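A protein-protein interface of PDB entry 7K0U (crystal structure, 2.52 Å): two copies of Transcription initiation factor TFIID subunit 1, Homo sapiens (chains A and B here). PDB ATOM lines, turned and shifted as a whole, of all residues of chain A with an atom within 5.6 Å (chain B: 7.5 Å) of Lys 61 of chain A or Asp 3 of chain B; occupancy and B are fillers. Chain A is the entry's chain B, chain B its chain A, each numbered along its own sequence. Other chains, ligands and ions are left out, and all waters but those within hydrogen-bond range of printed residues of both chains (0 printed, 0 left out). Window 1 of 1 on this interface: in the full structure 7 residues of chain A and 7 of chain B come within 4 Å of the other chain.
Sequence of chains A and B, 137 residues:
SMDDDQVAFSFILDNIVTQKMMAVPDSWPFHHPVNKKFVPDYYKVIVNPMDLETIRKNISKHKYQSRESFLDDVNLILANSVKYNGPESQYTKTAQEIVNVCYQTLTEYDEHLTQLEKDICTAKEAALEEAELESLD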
ATOM      1  N   ARG A  56     -22.611 -29.555  18.052  1.00  0.00           N
ATOM      2  CA  ARG A  56     -23.450 -29.331  16.875  1.00  0.00           C
ATOM      3  C   ARG A  56     -23.077 -28.038  16.149  1.00  0.00           C
ATOM      4  O   ARG A  56     -23.049 -28.001  14.908  1.00  0.00           O
ATOM      5  CB  ARG A  56     -24.930 -29.292  17.258  1.00  0.00           C
ATOM      6  CG  ARG A  56     -25.527 -30.563  17.890  1.00  0.00           C
ATOM      7  CD  ARG A  56     -27.049 -30.418  17.903  1.00  0.00           C
ATOM      8  NE  ARG A  56     -27.547 -30.489  16.531  1.00  0.00           N
ATOM      9  CZ  ARG A  56     -28.727 -30.037  16.109  1.00  0.00           C
ATOM     10  NH1 ARG A  56     -29.567 -29.424  16.948  1.00  0.00           N
ATOM     11  NH2 ARG A  56     -29.053 -30.176  14.818  1.00  0.00           N
ATOM     12  N   LYS A  57     -22.830 -26.954  16.896  1.00  0.00           N
ATOM     13  CA  LYS A  57     -22.397 -25.714  16.250  1.00  0.00           C
ATOM     14  C   LYS A  57     -21.089 -25.910  15.486  1.00  0.00           C
ATOM     15  O   LYS A  57     -20.958 -25.464  14.340  1.00  0.00           O
ATOM     16  CB  LYS A  57     -22.253 -24.586  17.275  1.00  0.00           C
ATOM     17  CG  LYS A  57     -23.566 -24.079  17.878  1.00  0.00           C
ATOM     18  CD  LYS A  57     -23.287 -22.984  18.886  1.00  0.00           C
ATOM     19  CE  LYS A  57     -24.514 -22.583  19.688  1.00  0.00           C
ATOM     20  NZ  LYS A  57     -25.478 -21.763  18.935  1.00  0.00           N
ATOM     21  N   ASN A  58     -20.119 -26.607  16.094  1.00  0.00           N
ATOM     22  CA  ASN A  58     -18.862 -26.884  15.402  1.00  0.00           C
ATOM     23  C   ASN A  58     -19.107 -27.642  14.109  1.00  0.00           C
ATOM     24  O   ASN A  58     -18.461 -27.372  13.090  1.00  0.00           O
ATOM     25  CB  ASN A  58     -17.926 -27.688  16.299  1.00  0.00           C
ATOM     26  CG  ASN A  58     -17.387 -26.897  17.464  1.00  0.00           C
ATOM     27  OD1 ASN A  58     -16.999 -25.734  17.332  1.00  0.00           O
ATOM     28  ND2 ASN A  58     -17.342 -27.536  18.615  1.00  0.00           N
ATOM     29  N   ILE A  59     -20.001 -28.631  14.156  1.00  0.00           N
ATOM     30  CA  ILE A  59     -20.401 -29.386  12.974  1.00  0.00           C
ATOM     31  C   ILE A  59     -20.978 -28.466  11.903  1.00  0.00           C
ATOM     32  O   ILE A  59     -20.631 -28.566  10.716  1.00  0.00           O
ATOM     33  CB  ILE A  59     -21.397 -30.481  13.396  1.00  0.00           C
ATOM     34  CG1 ILE A  59     -20.664 -31.542  14.206  1.00  0.00           C
ATOM     35  CG2 ILE A  59     -22.154 -31.047  12.213  1.00  0.00           C
ATOM     36  CD1 ILE A  59     -21.571 -32.440  14.947  1.00  0.00           C
ATOM     37  N   SER A  60     -21.848 -27.542  12.301  1.00  0.00           N
ATOM     38  CA  SER A  60     -22.448 -26.664  11.309  1.00  0.00           C
ATOM     39  C   SER A  60     -21.409 -25.715  10.713  1.00  0.00           C
ATOM     40  O   SER A  60     -21.538 -25.304   9.548  1.00  0.00           O
ATOM     41  CB  SER A  60     -23.641 -25.922  11.918  1.00  0.00           C
ATOM     42  OG  SER A  60     -23.259 -25.000  12.911  1.00  0.00           O
ATOM     43  N   LYS A  61     -20.350 -25.400  11.474  1.00  0.00           N
ATOM     44  CA  LYS A  61     -19.187 -24.673  10.967  1.00  0.00           C
ATOM     45  C   LYS A  61     -18.209 -25.580  10.219  1.00  0.00           C
ATOM     46  O   LYS A  61     -17.161 -25.098   9.779  1.00  0.00           O
ATOM     47  CB  LYS A  61     -18.439 -23.963  12.119  1.00  0.00           C
ATOM     48  CG  LYS A  61     -19.215 -22.845  12.834  1.00  0.00           C
ATOM     49  CD  LYS A  61     -18.320 -21.952  13.726  1.00  0.00           C
ATOM     50  CE  LYS A  61     -17.940 -22.547  15.112  1.00  0.00           C
ATOM     51  NZ  LYS A  61     -19.046 -22.521  16.140  1.00  0.00           N
ATOM     52  N   HIS A  62     -18.522 -26.875  10.091  1.00  0.00           N
ATOM     53  CA  HIS A  62     -17.635 -27.877   9.491  1.00  0.00           C
ATOM     54  C   HIS A  62     -16.278 -27.913  10.197  1.00  0.00           C
ATOM     55  O   HIS A  62     -15.239 -28.059   9.552  1.00  0.00           O
ATOM     56  CB  HIS A  62     -17.440 -27.661   7.984  1.00  0.00           C
ATOM     57  CG  HIS A  62     -18.719 -27.588   7.220  1.00  0.00           C
ATOM     58  ND1 HIS A  62     -19.609 -28.638   7.157  1.00  0.00           N
ATOM     59  CD2 HIS A  62     -19.246 -26.599   6.457  1.00  0.00           C
ATOM     60  CE1 HIS A  62     -20.645 -28.289   6.415  1.00  0.00           C
ATOM     61  NE2 HIS A  62     -20.445 -27.060   5.971  1.00  0.00           N
ATOM     62  N   LYS A  63     -16.274 -27.782  11.529  1.00  0.00           N
ATOM     63  CA  LYS A  63     -15.000 -27.788  12.249  1.00  0.00           C
ATOM     64  C   LYS A  63     -14.340 -29.161  12.197  1.00  0.00           C
ATOM     65  O   LYS A  63     -13.109 -29.258  12.136  1.00  0.00           O
ATOM     66  CB  LYS A  63     -15.167 -27.320  13.701  1.00  0.00           C
ATOM     67  CG  LYS A  63     -13.802 -27.122  14.409  1.00  0.00           C
ATOM     68  CD  LYS A  63     -13.848 -26.481  15.821  1.00  0.00           C
ATOM     69  CE  LYS A  63     -14.140 -27.463  16.954  1.00  0.00           C
ATOM     70  NZ  LYS A  63     -12.991 -28.354  17.253  1.00  0.00           N
ATOM     71  N   ASP B   3     -19.844 -16.787  16.208  1.00  0.00           N
ATOM     72  CA  ASP B   3     -19.806 -18.079  15.526  1.00  0.00           C
ATOM     73  C   ASP B   3     -21.141 -18.384  14.811  1.00  0.00           C
ATOM     74  O   ASP B   3     -21.174 -19.070  13.781  1.00  0.00           O
ATOM     75  CB  ASP B   3     -19.458 -19.199  16.533  1.00  0.00           C
ATOM     76  N   ASP B   4     -22.232 -17.802  15.320  1.00  0.00           N
ATOM     77  CA  ASP B   4     -23.561 -18.176  14.864  1.00  0.00           C
ATOM     78  C   ASP B   4     -23.940 -17.506  13.549  1.00  0.00           C
ATOM     79  O   ASP B   4     -24.865 -17.971  12.874  1.00  0.00           O
ATOM     80  CB  ASP B   4     -24.623 -17.768  15.914  1.00  0.00           C
ATOM     81  CG  ASP B   4     -24.570 -18.583  17.169  1.00  0.00           C
ATOM     82  OD1 ASP B   4     -24.136 -19.749  17.096  1.00  0.00           O
ATOM     83  OD2 ASP B   4     -24.988 -18.067  18.233  1.00  0.00           O
ATOM     84  N   ASP B   5     -23.243 -16.450  13.152  1.00  0.00           N
ATOM     85  CA  ASP B   5     -23.831 -15.549  12.172  1.00  0.00           C
ATOM     86  C   ASP B   5     -23.802 -16.154  10.763  1.00  0.00           C
ATOM     87  O   ASP B   5     -24.840 -16.251  10.097  1.00  0.00           O
ATOM     88  CB  ASP B   5     -23.107 -14.209  12.245  1.00  0.00           C
ATOM     89  CG  ASP B   5     -23.326 -13.503  13.569  1.00  0.00           C
ATOM     90  OD1 ASP B   5     -24.455 -13.546  14.126  1.00  0.00           O
ATOM     91  OD2 ASP B   5     -22.335 -12.950  14.085  1.00  0.00           O
ATOM     92  N   GLN B   6     -22.646 -16.667  10.341  1.00  0.00           N
ATOM     93  CA  GLN B   6     -22.560 -17.321   9.038  1.00  0.00           C
ATOM     94  C   GLN B   6     -23.520 -18.497   8.945  1.00  0.00           C
ATOM     95  O   GLN B   6     -24.256 -18.625   7.969  1.00  0.00           O
ATOM     96  CB  GLN B   6     -21.141 -17.808   8.777  1.00  0.00           C
ATOM     97  CG  GLN B   6     -21.081 -18.572   7.481  1.00  0.00           C
ATOM     98  CD  GLN B   6     -21.319 -17.643   6.253  1.00  0.00           C
ATOM     99  OE1 GLN B   6     -20.568 -16.696   6.021  1.00  0.00           O
ATOM    100  NE2 GLN B   6     -22.435 -17.853   5.562  1.00  0.00           N
ATOM    101  N   VAL B   7     -23.569 -19.336   9.976  1.00  0.00           N
ATOM    102  CA  VAL B   7     -24.508 -20.449   9.942  1.00  0.00           C
ATOM    103  C   VAL B   7     -25.928 -19.935   9.803  1.00  0.00           C
ATOM    104  O   VAL B   7     -26.734 -20.504   9.061  1.00  0.00           O
ATOM    105  CB  VAL B   7     -24.353 -21.325  11.197  1.00  0.00           C
ATOM    106  CG1 VAL B   7     -25.350 -22.466  11.187  1.00  0.00           C
ATOM    107  CG2 VAL B   7     -22.937 -21.857  11.309  1.00  0.00           C
ATOM    108  N   ALA B   8     -26.258 -18.860  10.525  1.00  0.00           N
ATOM    109  CA  ALA B   8     -27.619 -18.343  10.491  1.00  0.00           C
ATOM    110  C   ALA B   8     -27.957 -17.769   9.119  1.00  0.00           C
ATOM    111  O   ALA B   8     -29.056 -17.978   8.604  1.00  0.00           O
ATOM    112  CB  ALA B   8     -27.823 -17.302  11.597  1.00  0.00           C
ATOM    113  N   HIS B  62     -21.254 -22.711   2.850  1.00  0.00           N
ATOM    114  CA  HIS B  62     -21.079 -21.317   3.277  1.00  0.00           C
ATOM    115  C   HIS B  62     -20.321 -20.465   2.261  1.00  0.00           C
ATOM    116  O   HIS B  62     -19.509 -19.618   2.627  1.00  0.00           O
ATOM    117  CB  HIS B  62     -20.414 -21.248   4.643  1.00  0.00           C
ATOM    118  CG  HIS B  62     -21.130 -22.062   5.658  1.00  0.00           C
ATOM    119  ND1 HIS B  62     -22.473 -21.893   5.917  1.00  0.00           N
ATOM    120  CD2 HIS B  62     -20.702 -23.048   6.476  1.00  0.00           C
ATOM    121  CE1 HIS B  62     -22.846 -22.754   6.847  1.00  0.00           C
ATOM    122  NE2 HIS B  62     -21.788 -23.456   7.213  1.00  0.00           N
ATOM    123  N   ALA B 123     -16.364 -10.292  12.009  1.00  0.00           N
ATOM    124  CA  ALA B 123     -15.739 -11.461  12.626  1.00  0.00           C
ATOM    125  C   ALA B 123     -14.564 -11.960  11.796  1.00  0.00           C
ATOM    126  O   ALA B 123     -13.505 -12.275  12.347  1.00  0.00           O
ATOM    127  CB  ALA B 123     -16.765 -12.578  12.823  1.00  0.00           C
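A ring nitrogen (NE2) of His 62 of chain B is in hydrogen-bond range of the backbone carbonyl oxygen of Ser 60 of chain A, at 3.0 Å. The side-chain carboxylate of Asp 4 of chain B lies within salt-bridge range of the side-chain amino group of Lys 57 of chain A, at 3.0 Å.
His 62 of chain A touches its own counterpart, His 62 of chain B. Position printed for both chains: 62. Of the 5 pairs that touch across the chains among the printed residues, 1 has its exchanged pair printed and touching as well.
O of Lys 57 of chain A lies within hydrogen-bond range of OG of Ser 60 of chain A (2.7 Å).
Of chain B, only Val 7 (3.5 Å) and His 62 (3.0 Å) come within 4 Å of Ser 60 of chain A. Lys 61 of chain A touches just one residue of chain B: Asp 3. Of the printed residues of chain B, His 62 of chain A touches His 62 (3.8 Å). Asp 3 of chain B touches one residue of chain A. Of the printed residues of chain A, His 62 of chain B touches Ser 60 and His 62. The nearest residue of chain B that does not touch Lys 61 of chain A is Val 7 of chain B (4.1 Å). The nearest printed residue of chain A that does not touch Asp 3 of chain B is Lys 57 of chain A (5.9 Å). The nearest printed residue of chain A that does not touch His 62 of chain B is Lys 61 of chain A (4.7 Å).
Hydrophobic or aromatic side chains of chain B that line the printed part of chain A: Val 7 and His 62. Printed residues of chain A that touch a printed residue of chain B: Lys 57, Ser 60, Lys 61 and His 62. Hydrophobic or aromatic side chains of chain A that line the printed part of chain B: His 62. Among the printed residues, 5 pairs touch across the chains. Among the printed residues, Asp or Glu carboxylates within 4 Å of a Lys or Arg side-chain nitrogen of the other chain: Lys 57 of chain A with Asp 4 of chain B.
Among the printed residues, pairs that only touch across the chains: Ser 60 of chain A with Val 7 of chain B, Lys 61 of chain A with Asp 3 of chain B and His 62 of chain A with His 62 of chain B.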
